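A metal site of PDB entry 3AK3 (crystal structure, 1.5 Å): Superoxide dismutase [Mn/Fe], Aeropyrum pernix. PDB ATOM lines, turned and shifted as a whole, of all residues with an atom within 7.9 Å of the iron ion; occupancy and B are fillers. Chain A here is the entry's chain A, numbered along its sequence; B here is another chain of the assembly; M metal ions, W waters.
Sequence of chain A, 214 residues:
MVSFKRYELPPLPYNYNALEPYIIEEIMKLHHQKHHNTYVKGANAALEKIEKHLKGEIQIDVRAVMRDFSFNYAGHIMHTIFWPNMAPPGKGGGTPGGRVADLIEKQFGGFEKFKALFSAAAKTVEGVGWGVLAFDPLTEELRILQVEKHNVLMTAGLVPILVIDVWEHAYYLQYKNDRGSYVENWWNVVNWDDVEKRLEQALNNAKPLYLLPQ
Water W1 lies within hydrogen-bond range of OD1 of Asp 165 (3.0 Å), NE2 of His 150 (3.1 Å) and NE1 of Trp 167 (3.4 Å).
The backbone NH of Trp 167 is in hydrogen-bond range of the side-chain carboxylate of Asp 165. ND1 of His 169 lies within hydrogen-bond range of OE2 of Glu 168 of chain B, at 2.7 Å. NE1 of Trp 83 sits close to O of His 79, at 3.3 Å. O of Asp 165 sits at hydrogen-bond distance from OH of Tyr 182, 2.8 Å away. A ring nitrogen (ND1) of His 79 is in hydrogen-bond range of the backbone carbonyl oxygen (O) of Gly 75 (2.7 Å). The backbone carbonyl oxygen of His 31 lies within hydrogen-bond range of the backbone NH of His 36 (2.9 Å).
Of the 22 residues printed, 4 come within 4 Å of the iron ion. The nearest printed residue that does not touch the iron ion is Tyr 39 (4.4 Å).
The iron ion is bound by OD2 of Asp 165 (1.9 Å). Water W1 binds the iron ion, 2.1 Å away. A ring nitrogen (NE2) of His 79 binds the iron ion, at 2.1 Å. The iron ion is bound by NE2 of His 169 (2.2 Å). A ring nitrogen (NE2) of His 31 is bound to the iron ion (2.2 Å). Water W2 is bound to the iron ion, 2.2 Å away. The iron ion has six donor atoms within binding distance.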
ATOM      1  N   HIS A  31     -16.287   0.757   7.806  1.00  0.00           N
ATOM      2  CA  HIS A  31     -15.004   1.455   7.690  1.00  0.00           C
ATOM      3  C   HIS A  31     -14.210   0.912   6.519  1.00  0.00           C
ATOM      4  O   HIS A  31     -13.623   1.655   5.728  1.00  0.00           O
ATOM      5  CB  HIS A  31     -14.223   1.260   8.987  1.00  0.00           C
ATOM      6  CG  HIS A  31     -13.189   2.309   9.237  1.00  0.00           C
ATOM      7  ND1 HIS A  31     -12.448   2.345  10.396  1.00  0.00           N
ATOM      8  CD2 HIS A  31     -12.791   3.374   8.498  1.00  0.00           C
ATOM      9  CE1 HIS A  31     -11.616   3.376  10.346  1.00  0.00           C
ATOM     10  NE2 HIS A  31     -11.818   4.020   9.220  1.00  0.00           N
ATOM     11  N   HIS A  32     -14.200  -0.410   6.385  1.00  0.00           N
ATOM     12  CA  HIS A  32     -13.471  -1.072   5.324  1.00  0.00           C
ATOM     13  C   HIS A  32     -14.195  -0.984   3.973  1.00  0.00           C
ATOM     14  O   HIS A  32     -13.642  -0.483   2.990  1.00  0.00           O
ATOM     15  CB  HIS A  32     -13.208  -2.521   5.716  1.00  0.00           C
ATOM     16  CG  HIS A  32     -12.370  -3.272   4.727  1.00  0.00           C
ATOM     17  ND1 HIS A  32     -12.772  -4.468   4.184  1.00  0.00           N
ATOM     18  CD2 HIS A  32     -11.167  -2.988   4.179  1.00  0.00           C
ATOM     19  CE1 HIS A  32     -11.846  -4.901   3.352  1.00  0.00           C
ATOM     20  NE2 HIS A  32     -10.863  -4.018   3.321  1.00  0.00           N
ATOM     21  N   HIS A  35     -15.796   3.305   3.597  1.00  0.00           N
ATOM     22  CA  HIS A  35     -14.846   4.411   3.703  1.00  0.00           C
ATOM     23  C   HIS A  35     -13.527   4.143   2.997  1.00  0.00           C
ATOM     24  O   HIS A  35     -13.137   4.895   2.105  1.00  0.00           O
ATOM     25  CB  HIS A  35     -14.604   4.772   5.170  1.00  0.00           C
ATOM     26  CG  HIS A  35     -15.821   5.307   5.852  1.00  0.00           C
ATOM     27  ND1 HIS A  35     -16.210   6.628   5.752  1.00  0.00           N
ATOM     28  CD2 HIS A  35     -16.756   4.701   6.623  1.00  0.00           C
ATOM     29  CE1 HIS A  35     -17.327   6.812   6.440  1.00  0.00           C
ATOM     30  NE2 HIS A  35     -17.678   5.651   6.983  1.00  0.00           N
ATOM     31  N   HIS A  36     -12.846   3.074   3.370  1.00  0.00           N
ATOM     32  CA  HIS A  36     -11.576   2.771   2.731  1.00  0.00           C
ATOM     33  C   HIS A  36     -11.783   2.578   1.226  1.00  0.00           C
ATOM     34  O   HIS A  36     -11.046   3.161   0.413  1.00  0.00           O
ATOM     35  CB  HIS A  36     -10.852   1.606   3.404  1.00  0.00           C
ATOM     36  CG  HIS A  36      -9.424   1.456   2.957  1.00  0.00           C
ATOM     37  ND1 HIS A  36      -8.597   0.453   3.436  1.00  0.00           N
ATOM     38  CD2 HIS A  36      -8.684   2.157   2.077  1.00  0.00           C
ATOM     39  CE1 HIS A  36      -7.413   0.546   2.858  1.00  0.00           C
ATOM     40  NE2 HIS A  36      -7.436   1.576   2.024  1.00  0.00           N
ATOM     41  N   TYR A  39     -11.799   5.824  -0.745  1.00  0.00           N
ATOM     42  CA  TYR A  39     -10.492   6.429  -0.990  1.00  0.00           C
ATOM     43  C   TYR A  39      -9.768   5.774  -2.153  1.00  0.00           C
ATOM     44  O   TYR A  39      -9.216   6.471  -2.990  1.00  0.00           O
ATOM     45  CB  TYR A  39      -9.595   6.391   0.250  1.00  0.00           C
ATOM     46  CG  TYR A  39     -10.246   6.928   1.489  1.00  0.00           C
ATOM     47  CD1 TYR A  39     -10.867   8.169   1.502  1.00  0.00           C
ATOM     48  CD2 TYR A  39     -10.238   6.181   2.663  1.00  0.00           C
ATOM     49  CE1 TYR A  39     -11.474   8.661   2.667  1.00  0.00           C
ATOM     50  CE2 TYR A  39     -10.833   6.653   3.807  1.00  0.00           C
ATOM     51  CZ  TYR A  39     -11.436   7.882   3.818  1.00  0.00           C
ATOM     52  OH  TYR A  39     -12.015   8.328   4.981  1.00  0.00           O
ATOM     53  N   GLY A  75      -5.878   8.963   2.462  1.00  0.00           N
ATOM     54  CA  GLY A  75      -6.848   8.071   3.120  1.00  0.00           C
ATOM     55  C   GLY A  75      -6.478   6.607   2.878  1.00  0.00           C
ATOM     56  O   GLY A  75      -6.545   5.747   3.769  1.00  0.00           O
ATOM     57  N   MET A  78      -3.106   5.590   4.746  1.00  0.00           N
ATOM     58  CA  MET A  78      -3.272   5.629   6.205  1.00  0.00           C
ATOM     59  C   MET A  78      -4.093   4.436   6.694  1.00  0.00           C
ATOM     60  O   MET A  78      -3.736   3.823   7.682  1.00  0.00           O
ATOM     61  CB  MET A  78      -3.892   6.946   6.689  1.00  0.00           C
ATOM     62  CG  MET A  78      -3.058   8.198   6.440  1.00  0.00           C
ATOM     63  SD  MET A  78      -1.490   8.237   7.335  1.00  0.00           S
ATOM     64  CE  MET A  78      -2.057   8.591   9.011  1.00  0.00           C
ATOM     65  N   HIS A  79      -5.175   4.081   5.993  1.00  0.00           N
ATOM     66  CA  HIS A  79      -5.939   2.878   6.350  1.00  0.00           C
ATOM     67  C   HIS A  79      -5.166   1.585   6.060  1.00  0.00           C
ATOM     68  O   HIS A  79      -5.291   0.597   6.789  1.00  0.00           O
ATOM     69  CB  HIS A  79      -7.324   2.901   5.698  1.00  0.00           C
ATOM     70  CG  HIS A  79      -8.225   3.963   6.240  1.00  0.00           C
ATOM     71  ND1 HIS A  79      -8.177   5.277   5.815  1.00  0.00           N
ATOM     72  CD2 HIS A  79      -9.181   3.925   7.205  1.00  0.00           C
ATOM     73  CE1 HIS A  79      -9.049   5.995   6.496  1.00  0.00           C
ATOM     74  NE2 HIS A  79      -9.675   5.203   7.341  1.00  0.00           N
ATOM     75  N   PHE A  82      -3.238   1.355   9.118  1.00  0.00           N
ATOM     76  CA  PHE A  82      -4.171   1.170  10.233  1.00  0.00           C
ATOM     77  C   PHE A  82      -4.600  -0.286  10.495  1.00  0.00           C
ATOM     78  O   PHE A  82      -4.589  -0.736  11.637  1.00  0.00           O
ATOM     79  CB  PHE A  82      -5.389   2.050  10.003  1.00  0.00           C
ATOM     80  CG  PHE A  82      -6.376   2.077  11.151  1.00  0.00           C
ATOM     81  CD1 PHE A  82      -5.970   2.425  12.438  1.00  0.00           C
ATOM     82  CD2 PHE A  82      -7.717   1.797  10.916  1.00  0.00           C
ATOM     83  CE1 PHE A  82      -6.900   2.454  13.495  1.00  0.00           C
ATOM     84  CE2 PHE A  82      -8.660   1.840  11.961  1.00  0.00           C
ATOM     85  CZ  PHE A  82      -8.253   2.159  13.245  1.00  0.00           C
ATOM     86  N   TRP A  83      -5.007  -0.996   9.440  1.00  0.00           N
ATOM     87  CA  TRP A  83      -5.574  -2.336   9.644  1.00  0.00           C
ATOM     88  C   TRP A  83      -4.568  -3.335  10.224  1.00  0.00           C
ATOM     89  O   TRP A  83      -4.859  -3.976  11.245  1.00  0.00           O
ATOM     90  CB  TRP A  83      -6.209  -2.905   8.372  1.00  0.00           C
ATOM     91  CG  TRP A  83      -7.177  -2.006   7.646  1.00  0.00           C
ATOM     92  CD1 TRP A  83      -7.142  -1.690   6.331  1.00  0.00           C
ATOM     93  CD2 TRP A  83      -8.340  -1.350   8.191  1.00  0.00           C
ATOM     94  NE1 TRP A  83      -8.194  -0.873   6.016  1.00  0.00           N
ATOM     95  CE2 TRP A  83      -8.941  -0.646   7.127  1.00  0.00           C
ATOM     96  CE3 TRP A  83      -8.931  -1.290   9.469  1.00  0.00           C
ATOM     97  CZ2 TRP A  83     -10.105   0.109   7.290  1.00  0.00           C
ATOM     98  CZ3 TRP A  83     -10.077  -0.523   9.626  1.00  0.00           C
ATOM     99  CH2 TRP A  83     -10.653   0.170   8.548  1.00  0.00           C
ATOM    100  N   GLY A 129      -9.148  13.109  12.119  1.00  0.00           N
ATOM    101  CA  GLY A 129      -7.751  12.899  11.782  1.00  0.00           C
ATOM    102  C   GLY A 129      -7.178  11.659  12.417  1.00  0.00           C
ATOM    103  O   GLY A 129      -7.864  10.651  12.589  1.00  0.00           O
ATOM    104  N   TRP A 130      -5.894  11.744  12.753  1.00  0.00           N
ATOM    105  CA  TRP A 130      -5.085  10.593  13.123  1.00  0.00           C
ATOM    106  C   TRP A 130      -4.081  10.958  14.198  1.00  0.00           C
ATOM    107  O   TRP A 130      -3.498  12.064  14.191  1.00  0.00           O
ATOM    108  CB  TRP A 130      -4.275  10.079  11.910  1.00  0.00           C
ATOM    109  CG  TRP A 130      -5.086   9.666  10.756  1.00  0.00           C
ATOM    110  CD1 TRP A 130      -5.614  10.480   9.795  1.00  0.00           C
ATOM    111  CD2 TRP A 130      -5.461   8.323  10.413  1.00  0.00           C
ATOM    112  NE1 TRP A 130      -6.292   9.728   8.874  1.00  0.00           N
ATOM    113  CE2 TRP A 130      -6.239   8.403   9.231  1.00  0.00           C
ATOM    114  CE3 TRP A 130      -5.228   7.060  10.991  1.00  0.00           C
ATOM    115  CZ2 TRP A 130      -6.767   7.279   8.614  1.00  0.00           C
ATOM    116  CZ3 TRP A 130      -5.756   5.936  10.373  1.00  0.00           C
ATOM    117  CH2 TRP A 130      -6.523   6.055   9.203  1.00  0.00           C
ATOM    118  N   HIS A 150      -6.767  13.513   6.232  1.00  0.00           N
ATOM    119  CA  HIS A 150      -5.751  12.499   5.950  1.00  0.00           C
ATOM    120  C   HIS A 150      -4.455  13.129   5.518  1.00  0.00           C
ATOM    121  O   HIS A 150      -3.431  12.444   5.438  1.00  0.00           O
ATOM    122  CB  HIS A 150      -6.255  11.580   4.845  1.00  0.00           C
ATOM    123  CG  HIS A 150      -7.443  10.784   5.243  1.00  0.00           C
ATOM    124  ND1 HIS A 150      -8.552  10.605   4.432  1.00  0.00           N
ATOM    125  CD2 HIS A 150      -7.710  10.124   6.389  1.00  0.00           C
ATOM    126  CE1 HIS A 150      -9.445   9.863   5.068  1.00  0.00           C
ATOM    127  NE2 HIS A 150      -8.953   9.558   6.262  1.00  0.00           N
ATOM    128  N   ILE A 164      -3.558   5.761  14.684  1.00  0.00           N
ATOM    129  CA  ILE A 164      -4.923   5.544  15.156  1.00  0.00           C
ATOM    130  C   ILE A 164      -5.858   6.507  14.439  1.00  0.00           C
ATOM    131  O   ILE A 164      -5.642   7.725  14.437  1.00  0.00           O
ATOM    132  CB  ILE A 164      -5.059   5.657  16.702  1.00  0.00           C
ATOM    133  CG1 ILE A 164      -6.499   5.381  17.133  1.00  0.00           C
ATOM    134  CG2 ILE A 164      -4.575   7.017  17.228  1.00  0.00           C
ATOM    135  CD1 ILE A 164      -6.750   5.502  18.661  1.00  0.00           C
ATOM    136  N   ASP A 165      -6.897   5.941  13.824  1.00  0.00           N
ATOM    137  CA  ASP A 165      -7.939   6.714  13.163  1.00  0.00           C
ATOM    138  C   ASP A 165      -8.873   7.308  14.187  1.00  0.00           C
ATOM    139  O   ASP A 165      -9.519   6.573  14.931  1.00  0.00           O
ATOM    140  CB  ASP A 165      -8.709   5.795  12.223  1.00  0.00           C
ATOM    141  CG  ASP A 165      -9.658   6.536  11.278  1.00  0.00           C
ATOM    142  OD1 ASP A 165      -9.812   7.765  11.399  1.00  0.00           O
ATOM    143  OD2 ASP A 165     -10.231   5.881  10.362  1.00  0.00           O
ATOM    144  N   VAL A 166      -8.936   8.633  14.253  1.00  0.00           N
ATOM    145  CA  VAL A 166      -9.905   9.299  15.140  1.00  0.00           C
ATOM    146  C   VAL A 166     -10.919  10.131  14.345  1.00  0.00           C
ATOM    147  O   VAL A 166     -11.546  11.065  14.869  1.00  0.00           O
ATOM    148  CB  VAL A 166      -9.244  10.102  16.281  1.00  0.00           C
ATOM    149  CG1 VAL A 166      -8.592   9.167  17.300  1.00  0.00           C
ATOM    150  CG2 VAL A 166      -8.228  11.102  15.737  1.00  0.00           C
ATOM    151  N   TRP A 167     -11.112   9.774  13.086  1.00  0.00           N
ATOM    152  CA  TRP A 167     -12.313  10.186  12.411  1.00  0.00           C
ATOM    153  C   TRP A 167     -13.508   9.633  13.202  1.00  0.00           C
ATOM    154  O   TRP A 167     -13.402   8.565  13.839  1.00  0.00           O
ATOM    155  CB  TRP A 167     -12.347   9.669  10.986  1.00  0.00           C
ATOM    156  CG  TRP A 167     -11.449  10.413  10.034  1.00  0.00           C
ATOM    157  CD1 TRP A 167     -10.089  10.551  10.100  1.00  0.00           C
ATOM    158  CD2 TRP A 167     -11.877  11.099   8.855  1.00  0.00           C
ATOM    159  NE1 TRP A 167      -9.639  11.289   9.030  1.00  0.00           N
ATOM    160  CE2 TRP A 167     -10.712  11.633   8.244  1.00  0.00           C
ATOM    161  CE3 TRP A 167     -13.114  11.305   8.242  1.00  0.00           C
ATOM    162  CZ2 TRP A 167     -10.764  12.378   7.066  1.00  0.00           C
ATOM    163  CZ3 TRP A 167     -13.171  12.042   7.069  1.00  0.00           C
ATOM    164  CH2 TRP A 167     -11.994  12.573   6.485  1.00  0.00           C
ATOM    165  N   GLU A 168     -14.609  10.363  13.170  1.00  0.00           N
ATOM    166  CA  GLU A 168     -15.784   9.961  13.946  1.00  0.00           C
ATOM    167  C   GLU A 168     -16.306   8.606  13.497  1.00  0.00           C
ATOM    168  O   GLU A 168     -16.746   7.804  14.321  1.00  0.00           O
ATOM    169  CB  GLU A 168     -16.870  11.046  13.881  1.00  0.00           C
ATOM    170  CG  GLU A 168     -16.414  12.364  14.529  1.00  0.00           C
ATOM    171  CD  GLU A 168     -17.423  13.485  14.448  1.00  0.00           C
ATOM    172  OE1 GLU A 168     -18.077  13.683  13.394  1.00  0.00           O
ATOM    173  OE2 GLU A 168     -17.551  14.203  15.452  1.00  0.00           O
ATOM    174  N   HIS A 169     -16.219   8.316  12.199  1.00  0.00           N
ATOM    175  CA  HIS A 169     -16.676   7.024  11.703  1.00  0.00           C
ATOM    176  C   HIS A 169     -15.936   5.835  12.310  1.00  0.00           C
ATOM    177  O   HIS A 169     -16.430   4.704  12.235  1.00  0.00           O
ATOM    178  CB  HIS A 169     -16.619   6.953  10.169  1.00  0.00           C
ATOM    179  CG  HIS A 169     -15.237   7.057   9.593  1.00  0.00           C
ATOM    180  ND1 HIS A 169     -14.860   8.082   8.745  1.00  0.00           N
ATOM    181  CD2 HIS A 169     -14.156   6.253   9.721  1.00  0.00           C
ATOM    182  CE1 HIS A 169     -13.601   7.903   8.384  1.00  0.00           C
ATOM    183  NE2 HIS A 169     -13.144   6.804   8.960  1.00  0.00           N
ATOM    184  N   ALA A 170     -14.754   6.084  12.876  1.00  0.00           N
ATOM    185  CA  ALA A 170     -13.951   5.035  13.492  1.00  0.00           C
ATOM    186  C   ALA A 170     -14.497   4.582  14.844  1.00  0.00           C
ATOM    187  O   ALA A 170     -14.164   3.484  15.296  1.00  0.00           O
ATOM    188  CB  ALA A 170     -12.477   5.448  13.603  1.00  0.00           C
ATOM    189  N   TYR A 182     -12.667   5.486  23.308  1.00  0.00           N
ATOM    190  CA  TYR A 182     -12.244   4.740  22.125  1.00  0.00           C
ATOM    191  C   TYR A 182     -10.731   4.607  22.075  1.00  0.00           C
ATOM    192  O   TYR A 182     -10.218   3.512  21.867  1.00  0.00           O
ATOM    193  CB  TYR A 182     -12.771   5.404  20.853  1.00  0.00           C
ATOM    194  CG  TYR A 182     -12.024   5.029  19.587  1.00  0.00           C
ATOM    195  CD1 TYR A 182     -12.066   3.736  19.076  1.00  0.00           C
ATOM    196  CD2 TYR A 182     -11.312   6.001  18.884  1.00  0.00           C
ATOM    197  CE1 TYR A 182     -11.392   3.410  17.903  1.00  0.00           C
ATOM    198  CE2 TYR A 182     -10.638   5.681  17.719  1.00  0.00           C
ATOM    199  CZ  TYR A 182     -10.687   4.391  17.229  1.00  0.00           C
ATOM    200  OH  TYR A 182     -10.023   4.056  16.073  1.00  0.00           O
ATOM    201  N   GLU B 168     -19.638  14.014  10.526  1.00  0.00           N
ATOM    202  CA  GLU B 168     -20.139  12.648  10.646  1.00  0.00           C
ATOM    203  C   GLU B 168     -21.100  12.477  11.822  1.00  0.00           C
ATOM    204  O   GLU B 168     -22.125  11.802  11.695  1.00  0.00           O
ATOM    205  CB  GLU B 168     -18.978  11.653  10.694  1.00  0.00           C
ATOM    206  CG  GLU B 168     -18.192  11.604   9.393  1.00  0.00           C
ATOM    207  CD  GLU B 168     -17.017  10.655   9.424  1.00  0.00           C
ATOM    208  OE1 GLU B 168     -16.342  10.554  10.463  1.00  0.00           O
ATOM    209  OE2 GLU B 168     -16.775  10.009   8.372  1.00  0.00           O
HETATM  210 FE    FE M   1     -11.138   6.023   8.676  1.00  0.00          FE
HETATM  211  O   HOH W   1     -10.375   7.971   8.494  1.00  0.00           O
HETATM  212  O   HOH W   2     -12.095   5.987   6.668  1.00  0.00           O
